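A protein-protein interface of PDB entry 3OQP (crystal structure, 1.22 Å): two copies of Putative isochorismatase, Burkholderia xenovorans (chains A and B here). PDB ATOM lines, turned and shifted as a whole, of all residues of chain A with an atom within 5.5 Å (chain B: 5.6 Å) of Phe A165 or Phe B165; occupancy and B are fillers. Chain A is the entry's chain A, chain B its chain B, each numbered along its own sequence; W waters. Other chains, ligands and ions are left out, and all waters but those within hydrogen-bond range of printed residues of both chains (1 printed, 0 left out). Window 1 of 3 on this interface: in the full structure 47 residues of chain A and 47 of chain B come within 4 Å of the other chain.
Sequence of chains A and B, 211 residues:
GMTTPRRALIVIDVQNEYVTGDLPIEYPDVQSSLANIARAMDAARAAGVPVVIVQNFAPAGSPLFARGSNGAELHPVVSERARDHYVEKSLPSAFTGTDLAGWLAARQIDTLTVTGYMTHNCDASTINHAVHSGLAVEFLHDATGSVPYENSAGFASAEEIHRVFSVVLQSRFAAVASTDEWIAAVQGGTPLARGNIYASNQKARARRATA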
ATOM      1  N   THR A 119      13.969  23.426  30.092  1.00  0.00           N
ATOM      2  CA  THR A 119      13.324  22.660  28.977  1.00  0.00           C
ATOM      3  C   THR A 119      14.260  21.533  28.470  1.00  0.00           C
ATOM      4  O   THR A 119      13.903  20.355  28.408  1.00  0.00           O
ATOM      5  CB  THR A 119      12.943  23.548  27.819  1.00  0.00           C
ATOM      6  OG1 THR A 119      11.907  24.392  28.299  1.00  0.00           O
ATOM      7  CG2 THR A 119      12.498  22.709  26.664  1.00  0.00           C
ATOM      8  N   HIS A 120      15.472  21.925  28.117  1.00  0.00           N
ATOM      9  CA  HIS A 120      16.453  21.111  27.411  1.00  0.00           C
ATOM     10  C   HIS A 120      17.404  20.280  28.270  1.00  0.00           C
ATOM     11  O   HIS A 120      18.237  19.583  27.688  1.00  0.00           O
ATOM     12  CB  HIS A 120      17.229  22.061  26.492  1.00  0.00           C
ATOM     13  CG  HIS A 120      17.929  23.105  27.265  1.00  0.00           C
ATOM     14  ND1 HIS A 120      17.308  24.288  27.619  1.00  0.00           N
ATOM     15  CD2 HIS A 120      19.166  23.127  27.796  1.00  0.00           C
ATOM     16  CE1 HIS A 120      18.152  24.960  28.416  1.00  0.00           C
ATOM     17  NE2 HIS A 120      19.295  24.283  28.510  1.00  0.00           N
ATOM     18  N   ASN A 121      17.260  20.355  29.573  1.00  0.00           N
ATOM     19  CA  ASN A 121      18.224  19.739  30.427  1.00  0.00           C
ATOM     20  C   ASN A 121      17.476  18.922  31.468  1.00  0.00           C
ATOM     21  O   ASN A 121      17.238  17.722  31.256  1.00  0.00           O
ATOM     22  CB  ASN A 121      19.153  20.821  31.009  1.00  0.00           C
ATOM     23  CG  ASN A 121      20.419  20.258  31.633  1.00  0.00           C
ATOM     24  OD1 ASN A 121      21.377  19.989  30.955  1.00  0.00           O
ATOM     25  ND2 ASN A 121      20.438  20.101  32.958  1.00  0.00           N
ATOM     26  N   ALA A 124      13.936  17.720  29.933  1.00  0.00           N
ATOM     27  CA  ALA A 124      14.058  16.711  28.885  1.00  0.00           C
ATOM     28  C   ALA A 124      14.612  15.383  29.446  1.00  0.00           C
ATOM     29  O   ALA A 124      14.156  14.312  28.986  1.00  0.00           O
ATOM     30  CB  ALA A 124      14.942  17.239  27.700  1.00  0.00           C
ATOM     31  N   GLU A 160      15.310  29.311  20.231  1.00  0.00           N
ATOM     32  CA  GLU A 160      15.560  28.188  19.324  1.00  0.00           C
ATOM     33  C   GLU A 160      15.588  26.888  20.148  1.00  0.00           C
ATOM     34  O   GLU A 160      15.025  25.870  19.764  1.00  0.00           O
ATOM     35  CB  GLU A 160      16.879  28.314  18.574  1.00  0.00           C
ATOM     36  CG  GLU A 160      16.927  29.280  17.455  1.00  0.00           C
ATOM     37  CD  GLU A 160      18.308  29.414  16.855  1.00  0.00           C
ATOM     38  OE1 GLU A 160      19.314  29.500  17.631  1.00  0.00           O
ATOM     39  OE2 GLU A 160      18.391  29.490  15.608  1.00  0.00           O
ATOM     40  N   ILE A 161      16.270  26.910  21.285  1.00  0.00           N
ATOM     41  CA  ILE A 161      16.379  25.706  22.129  1.00  0.00           C
ATOM     42  C   ILE A 161      14.965  25.274  22.579  1.00  0.00           C
ATOM     43  O   ILE A 161      14.618  24.108  22.494  1.00  0.00           O
ATOM     44  CB  ILE A 161      17.341  25.890  23.305  1.00  0.00           C
ATOM     45  CG1 ILE A 161      18.748  26.130  22.780  1.00  0.00           C
ATOM     46  CG2 ILE A 161      17.258  24.664  24.267  1.00  0.00           C
ATOM     47  CD1 ILE A 161      19.779  26.450  23.821  1.00  0.00           C
ATOM     48  N   HIS A 162      14.203  26.183  23.157  1.00  0.00           N
ATOM     49  CA  HIS A 162      12.909  25.867  23.679  1.00  0.00           C
ATOM     50  C   HIS A 162      11.950  25.387  22.621  1.00  0.00           C
ATOM     51  O   HIS A 162      11.222  24.424  22.816  1.00  0.00           O
ATOM     52  CB  HIS A 162      12.338  27.059  24.449  1.00  0.00           C
ATOM     53  CG  HIS A 162      11.010  26.809  25.082  1.00  0.00           C
ATOM     54  ND1 HIS A 162      10.853  26.105  26.257  1.00  0.00           N
ATOM     55  CD2 HIS A 162       9.781  27.203  24.695  1.00  0.00           C
ATOM     56  CE1 HIS A 162       9.564  26.104  26.564  1.00  0.00           C
ATOM     57  NE2 HIS A 162       8.895  26.766  25.641  1.00  0.00           N
ATOM     58  N   ARG A 163      11.978  26.059  21.477  1.00  0.00           N
ATOM     59  CA  ARG A 163      11.154  25.655  20.348  1.00  0.00           C
ATOM     60  C   ARG A 163      11.518  24.270  19.811  1.00  0.00           C
ATOM     61  O   ARG A 163      10.624  23.421  19.564  1.00  0.00           O
ATOM     62  CB  ARG A 163      11.155  26.688  19.235  1.00  0.00           C
ATOM     63  CG  ARG A 163      10.385  26.286  17.994  1.00  0.00           C
ATOM     64  CD  ARG A 163      10.055  27.404  16.989  1.00  0.00           C
ATOM     65  NE  ARG A 163      11.247  28.219  16.770  1.00  0.00           N
ATOM     66  CZ  ARG A 163      12.240  27.933  15.935  1.00  0.00           C
ATOM     67  NH1 ARG A 163      12.180  26.900  15.128  1.00  0.00           N
ATOM     68  NH2 ARG A 163      13.305  28.716  15.897  1.00  0.00           N
ATOM     69  N   VAL A 164      12.779  24.071  19.522  1.00  0.00           N
ATOM     70  CA  VAL A 164      13.260  22.780  19.059  1.00  0.00           C
ATOM     71  C   VAL A 164      12.788  21.680  20.004  1.00  0.00           C
ATOM     72  O   VAL A 164      12.286  20.680  19.597  1.00  0.00           O
ATOM     73  CB  VAL A 164      14.767  22.767  18.794  1.00  0.00           C
ATOM     74  CG1 VAL A 164      15.297  21.326  18.822  1.00  0.00           C
ATOM     75  CG2 VAL A 164      15.089  23.440  17.453  1.00  0.00           C
ATOM     76  N   PHE A 165      13.050  21.847  21.302  1.00  0.00           N
ATOM     77  CA  PHE A 165      12.673  20.827  22.253  1.00  0.00           C
ATOM     78  C   PHE A 165      11.163  20.651  22.308  1.00  0.00           C
ATOM     79  O   PHE A 165      10.680  19.515  22.360  1.00  0.00           O
ATOM     80  CB  PHE A 165      13.313  21.058  23.653  1.00  0.00           C
ATOM     81  CG  PHE A 165      14.670  20.443  23.790  1.00  0.00           C
ATOM     82  CD1 PHE A 165      15.778  21.039  23.248  1.00  0.00           C
ATOM     83  CD2 PHE A 165      14.799  19.226  24.464  1.00  0.00           C
ATOM     84  CE1 PHE A 165      17.002  20.463  23.344  1.00  0.00           C
ATOM     85  CE2 PHE A 165      16.035  18.665  24.585  1.00  0.00           C
ATOM     86  CZ  PHE A 165      17.122  19.272  24.015  1.00  0.00           C
ATOM     87  N   SER A 166      10.385  21.730  22.225  1.00  0.00           N
ATOM     88  CA  SER A 166       8.944  21.619  22.251  1.00  0.00           C
ATOM     89  C   SER A 166       8.432  20.807  21.058  1.00  0.00           C
ATOM     90  O   SER A 166       7.588  19.952  21.210  1.00  0.00           O
ATOM     91  CB  SER A 166       8.297  23.011  22.208  1.00  0.00           C
ATOM     92  OG  SER A 166       8.597  23.755  23.377  1.00  0.00           O
ATOM     93  N   VAL A 167       8.984  21.102  19.880  1.00  0.00           N
ATOM     94  CA  VAL A 167       8.590  20.386  18.670  1.00  0.00           C
ATOM     95  C   VAL A 167       9.008  18.902  18.648  1.00  0.00           C
ATOM     96  O   VAL A 167       8.256  17.995  18.356  1.00  0.00           O
ATOM     97  CB  VAL A 167       9.097  21.168  17.422  1.00  0.00           C
ATOM     98  CG1 VAL A 167       8.868  20.380  16.182  1.00  0.00           C
ATOM     99  CG2 VAL A 167       8.420  22.588  17.370  1.00  0.00           C
ATOM    100  N   VAL A 168      10.242  18.662  19.117  1.00  0.00           N
ATOM    101  CA  VAL A 168      10.721  17.290  19.232  1.00  0.00           C
ATOM    102  C   VAL A 168       9.924  16.522  20.278  1.00  0.00           C
ATOM    103  O   VAL A 168       9.519  15.388  20.060  1.00  0.00           O
ATOM    104  CB  VAL A 168      12.217  17.251  19.521  1.00  0.00           C
ATOM    105  CG1 VAL A 168      12.715  15.834  19.890  1.00  0.00           C
ATOM    106  CG2 VAL A 168      13.021  17.732  18.315  1.00  0.00           C
ATOM    107  N   LEU A 169       9.628  17.163  21.381  1.00  0.00           N
ATOM    108  CA  LEU A 169       8.830  16.476  22.408  1.00  0.00           C
ATOM    109  C   LEU A 169       7.476  16.081  21.824  1.00  0.00           C
ATOM    110  O   LEU A 169       6.996  14.963  22.013  1.00  0.00           O
ATOM    111  CB  LEU A 169       8.645  17.339  23.614  1.00  0.00           C
ATOM    112  CG  LEU A 169       9.884  17.430  24.517  1.00  0.00           C
ATOM    113  CD1 LEU A 169       9.610  18.553  25.533  1.00  0.00           C
ATOM    114  CD2 LEU A 169      10.254  16.146  25.227  1.00  0.00           C
ATOM    115  N   GLN A 170       6.819  17.021  21.160  1.00  0.00           N
ATOM    116  CA  GLN A 170       5.488  16.756  20.567  1.00  0.00           C
ATOM    117  C   GLN A 170       5.525  15.633  19.553  1.00  0.00           C
ATOM    118  O   GLN A 170       4.535  14.900  19.394  1.00  0.00           O
ATOM    119  CB  GLN A 170       4.875  18.031  20.018  1.00  0.00           C
ATOM    120  CG  GLN A 170       3.513  17.860  19.411  1.00  0.00           C
ATOM    121  CD  GLN A 170       2.421  17.511  20.395  1.00  0.00           C
ATOM    122  OE1 GLN A 170       2.635  17.558  21.587  1.00  0.00           O
ATOM    123  NE2 GLN A 170       1.251  17.150  19.907  1.00  0.00           N
ATOM    124  N   THR B 119      19.745  12.507  15.572  1.00  0.00           N
ATOM    125  CA  THR B 119      20.395  13.274  16.624  1.00  0.00           C
ATOM    126  C   THR B 119      19.463  13.513  17.823  1.00  0.00           C
ATOM    127  O   THR B 119      19.819  13.296  18.979  1.00  0.00           O
ATOM    128  CB  THR B 119      20.811  14.639  16.086  1.00  0.00           C
ATOM    129  OG1 THR B 119      21.818  14.440  15.082  1.00  0.00           O
ATOM    130  CG2 THR B 119      21.290  15.612  17.157  1.00  0.00           C
ATOM    131  N   HIS B 120      18.235  13.928  17.599  1.00  0.00           N
ATOM    132  CA  HIS B 120      17.305  14.445  18.570  1.00  0.00           C
ATOM    133  C   HIS B 120      16.352  13.410  19.140  1.00  0.00           C
ATOM    134  O   HIS B 120      15.524  13.743  19.978  1.00  0.00           O
ATOM    135  CB  HIS B 120      16.497  15.561  17.868  1.00  0.00           C
ATOM    136  CG  HIS B 120      15.754  15.081  16.651  1.00  0.00           C
ATOM    137  ND1 HIS B 120      16.332  14.971  15.397  1.00  0.00           N
ATOM    138  CD2 HIS B 120      14.531  14.517  16.561  1.00  0.00           C
ATOM    139  CE1 HIS B 120      15.451  14.421  14.577  1.00  0.00           C
ATOM    140  NE2 HIS B 120      14.343  14.160  15.245  1.00  0.00           N
ATOM    141  N   ASN B 121      16.453  12.173  18.694  1.00  0.00           N
ATOM    142  CA  ASN B 121      15.505  11.125  19.048  1.00  0.00           C
ATOM    143  C   ASN B 121      16.271   9.916  19.569  1.00  0.00           C
ATOM    144  O   ASN B 121      16.587   9.855  20.780  1.00  0.00           O
ATOM    145  CB  ASN B 121      14.556  10.858  17.842  1.00  0.00           C
ATOM    146  CG  ASN B 121      13.322  10.064  18.205  1.00  0.00           C
ATOM    147  OD1 ASN B 121      12.366  10.626  18.694  1.00  0.00           O
ATOM    148  ND2 ASN B 121      13.363   8.744  18.026  1.00  0.00           N
ATOM    149  N   ALA B 124      19.865  11.186  21.122  1.00  0.00           N
ATOM    150  CA  ALA B 124      19.729  11.927  22.407  1.00  0.00           C
ATOM    151  C   ALA B 124      19.206  11.037  23.516  1.00  0.00           C
ATOM    152  O   ALA B 124      19.712  11.116  24.658  1.00  0.00           O
ATOM    153  CB  ALA B 124      18.823  13.146  22.213  1.00  0.00           C
ATOM    154  N   GLU B 160      18.146  23.403  12.499  1.00  0.00           N
ATOM    155  CA  GLU B 160      17.891  23.940  13.847  1.00  0.00           C
ATOM    156  C   GLU B 160      17.932  22.835  14.904  1.00  0.00           C
ATOM    157  O   GLU B 160      18.488  23.018  15.969  1.00  0.00           O
ATOM    158  CB  GLU B 160      16.527  24.665  13.878  1.00  0.00           C
ATOM    159  CG  GLU B 160      16.514  26.051  13.254  1.00  0.00           C
ATOM    160  CD  GLU B 160      15.076  26.621  13.256  1.00  0.00           C
ATOM    161  OE1 GLU B 160      14.089  25.888  12.937  1.00  0.00           O
ATOM    162  OE2 GLU B 160      14.935  27.812  13.572  1.00  0.00           O
ATOM    163  N   ILE B 161      17.282  21.729  14.609  1.00  0.00           N
ATOM    164  CA  ILE B 161      17.176  20.615  15.535  1.00  0.00           C
ATOM    165  C   ILE B 161      18.578  20.064  15.786  1.00  0.00           C
ATOM    166  O   ILE B 161      19.006  19.936  16.927  1.00  0.00           O
ATOM    167  CB  ILE B 161      16.227  19.555  15.007  1.00  0.00           C
ATOM    168  CG1 ILE B 161      14.792  20.089  15.011  1.00  0.00           C
ATOM    169  CG2 ILE B 161      16.281  18.328  15.922  1.00  0.00           C
ATOM    170  CD1 ILE B 161      13.815  19.207  14.267  1.00  0.00           C
ATOM    171  N   HIS B 162      19.355  19.795  14.747  1.00  0.00           N
ATOM    172  CA  HIS B 162      20.677  19.217  14.938  1.00  0.00           C
ATOM    173  C   HIS B 162      21.609  20.168  15.647  1.00  0.00           C
ATOM    174  O   HIS B 162      22.370  19.737  16.531  1.00  0.00           O
ATOM    175  CB  HIS B 162      21.238  18.802  13.588  1.00  0.00           C
ATOM    176  CG  HIS B 162      22.574  18.156  13.633  1.00  0.00           C
ATOM    177  ND1 HIS B 162      22.760  16.828  13.974  1.00  0.00           N
ATOM    178  CD2 HIS B 162      23.789  18.655  13.336  1.00  0.00           C
ATOM    179  CE1 HIS B 162      24.062  16.562  13.902  1.00  0.00           C
ATOM    180  NE2 HIS B 162      24.704  17.641  13.504  1.00  0.00           N
ATOM    181  N   ARG B 163      21.587  21.447  15.302  1.00  0.00           N
ATOM    182  CA  ARG B 163      22.424  22.406  15.946  1.00  0.00           C
ATOM    183  C   ARG B 163      22.045  22.581  17.423  1.00  0.00           C
ATOM    184  O   ARG B 163      22.914  22.578  18.311  1.00  0.00           O
ATOM    185  CB  ARG B 163      22.352  23.742  15.173  1.00  0.00           C
ATOM    186  CG  ARG B 163      23.046  24.855  15.970  1.00  0.00           C
ATOM    187  CD  ARG B 163      23.318  26.079  15.073  1.00  0.00           C
ATOM    188  NE  ARG B 163      22.104  26.516  14.391  1.00  0.00           N
ATOM    189  CZ  ARG B 163      21.139  27.233  14.935  1.00  0.00           C
ATOM    190  NH1 ARG B 163      21.251  27.728  16.146  1.00  0.00           N
ATOM    191  NH2 ARG B 163      20.039  27.479  14.247  1.00  0.00           N
ATOM    192  N   VAL B 164      20.778  22.759  17.714  1.00  0.00           N
ATOM    193  CA  VAL B 164      20.345  22.933  19.090  1.00  0.00           C
ATOM    194  C   VAL B 164      20.773  21.710  19.909  1.00  0.00           C
ATOM    195  O   VAL B 164      21.376  21.851  21.005  1.00  0.00           O
ATOM    196  CB  VAL B 164      18.829  23.148  19.210  1.00  0.00           C
ATOM    197  CG1 VAL B 164      18.291  22.722  20.596  1.00  0.00           C
ATOM    198  CG2 VAL B 164      18.485  24.583  18.935  1.00  0.00           C
ATOM    199  N   PHE B 165      20.524  20.501  19.385  1.00  0.00           N
ATOM    200  CA  PHE B 165      20.935  19.325  20.172  1.00  0.00           C
ATOM    201  C   PHE B 165      22.452  19.226  20.278  1.00  0.00           C
ATOM    202  O   PHE B 165      22.953  18.865  21.335  1.00  0.00           O
ATOM    203  CB  PHE B 165      20.311  18.051  19.559  1.00  0.00           C
ATOM    204  CG  PHE B 165      18.990  17.736  20.134  1.00  0.00           C
ATOM    205  CD1 PHE B 165      17.842  18.390  19.674  1.00  0.00           C
ATOM    206  CD2 PHE B 165      18.851  16.817  21.159  1.00  0.00           C
ATOM    207  CE1 PHE B 165      16.628  18.122  20.259  1.00  0.00           C
ATOM    208  CE2 PHE B 165      17.651  16.557  21.704  1.00  0.00           C
ATOM    209  CZ  PHE B 165      16.558  17.166  21.303  1.00  0.00           C
ATOM    210  N   SER B 166      23.228  19.576  19.246  1.00  0.00           N
ATOM    211  CA  SER B 166      24.679  19.524  19.336  1.00  0.00           C
ATOM    212  C   SER B 166      25.145  20.499  20.413  1.00  0.00           C
ATOM    213  O   SER B 166      26.029  20.162  21.204  1.00  0.00           O
ATOM    214  CB  SER B 166      25.333  19.934  18.016  1.00  0.00           C
ATOM    215  OG  SER B 166      25.008  19.040  16.950  1.00  0.00           O
ATOM    216  N   VAL B 167      24.630  21.726  20.459  1.00  0.00           N
ATOM    217  CA  VAL B 167      25.018  22.699  21.445  1.00  0.00           C
ATOM    218  C   VAL B 167      24.607  22.280  22.863  1.00  0.00           C
ATOM    219  O   VAL B 167      25.400  22.406  23.803  1.00  0.00           O
ATOM    220  CB  VAL B 167      24.474  24.089  21.065  1.00  0.00           C
ATOM    221  CG1 VAL B 167      24.788  25.096  22.159  1.00  0.00           C
ATOM    222  CG2 VAL B 167      25.109  24.545  19.717  1.00  0.00           C
ATOM    223  N   VAL B 168      23.380  21.809  23.039  1.00  0.00           N
ATOM    224  CA  VAL B 168      22.963  21.332  24.361  1.00  0.00           C
ATOM    225  C   VAL B 168      23.761  20.098  24.817  1.00  0.00           C
ATOM    226  O   VAL B 168      24.202  20.049  25.997  1.00  0.00           O
ATOM    227  CB  VAL B 168      21.446  20.997  24.353  1.00  0.00           C
ATOM    228  CG1 VAL B 168      21.031  20.214  25.572  1.00  0.00           C
ATOM    229  CG2 VAL B 168      20.628  22.303  24.189  1.00  0.00           C
ATOM    230  N   LEU B 169      24.064  19.205  23.876  1.00  0.00           N
ATOM    231  CA  LEU B 169      24.877  18.058  24.308  1.00  0.00           C
ATOM    232  C   LEU B 169      26.240  18.524  24.761  1.00  0.00           C
ATOM    233  O   LEU B 169      26.699  18.036  25.765  1.00  0.00           O
ATOM    234  CB  LEU B 169      25.004  17.071  23.100  1.00  0.00           C
ATOM    235  CG  LEU B 169      23.779  16.203  22.794  1.00  0.00           C
ATOM    236  CD1 LEU B 169      23.907  15.523  21.429  1.00  0.00           C
ATOM    237  CD2 LEU B 169      23.473  15.239  23.962  1.00  0.00           C
ATOM    238  N   GLN B 170      26.873  19.444  24.066  1.00  0.00           N
ATOM    239  CA  GLN B 170      28.221  19.929  24.456  1.00  0.00           C
ATOM    240  C   GLN B 170      28.187  20.619  25.800  1.00  0.00           C
ATOM    241  O   GLN B 170      29.189  20.632  26.546  1.00  0.00           O
ATOM    242  CB  GLN B 170      28.774  20.837  23.364  1.00  0.00           C
ATOM    243  CG  GLN B 170      30.168  21.378  23.624  1.00  0.00           C
ATOM    244  CD  GLN B 170      31.257  20.301  23.705  1.00  0.00           C
ATOM    245  OE1 GLN B 170      31.026  19.152  23.431  1.00  0.00           O
ATOM    246  NE2 GLN B 170      32.440  20.693  24.190  1.00  0.00           N
HETATM  247  O   HOH W   1      16.490  29.689  13.764  1.00  0.00           O
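Among the printed residues, merely in contact across the chains: Phe A165 with Phe B165, Val A168 with His B120, His A120 with Val B168, Val A164 with Glu B160, Val A164 with Val B164, Val A164 with Phe B165, Glu A160 with Val B164, Phe A165 with Val B164, Val A164 with Ile B161 and Ile A161 with Val B164.
Of the 15 printed residues of chain B, 7 touch a printed residue of chain A.
Of the 15 printed residues of chain A, 7 touch a printed residue of chain B.
Printed residues of chain A that touch a printed residue of chain B: His A120, Glu A160, Ile A161, Arg A163, Val A164, Phe A165 and Val A168.
Among the printed residues, 12 pairs touch across the chains.
The side-chain carboxylate of Glu B160 is in salt-bridge range of the guanidinium group of Arg A163, at 3.0 Å.
The side-chain carboxylate of Glu A160 is in salt-bridge range of the guanidinium group of Arg B163, 2.9 Å away.
Phe A165 touches just these residues of chain B: Val B164 and Phe B165.
Phe B165 touches just these residues of chain A: Val A164 and Phe A165.
Of the printed residues of chain B, Ile A161 touches Val B164.
Printed residues of chain A within 4 Å of His B120: Val A168.
Printed residues of chain B within 4 Å of Glu A160: Arg B163 (2.9 Å) and Val B164 (3.8 Å).
Of the printed residues of chain A, Ile B161 touches Val A164.
Printed residues of chain B within 4 Å of Val A168: His B120 (3.5 Å).
The nearest residue of chain B that does not touch Phe A165 is Val B168 (4.2 Å).
The nearest residue of chain A that does not touch Phe B165 is Val A168 (4.1 Å).
The nearest printed residue of chain A that does not touch Arg B163 is Val A164 (7.0 Å).
Glu A160 touches Arg B163, and with the chains exchanged Arg A163 touches Glu B160.
Glu A160 touches Val B164, and with the chains exchanged Val A164 touches Glu B160.
Ile A161 touches Val B164, and with the chains exchanged Val A164 touches Ile B161.
Phe A165 touches its own counterpart, Phe B165.
Water W1 bridges the side-chain carboxylate of Glu B160 and the side-chain carboxylate of Glu A160.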
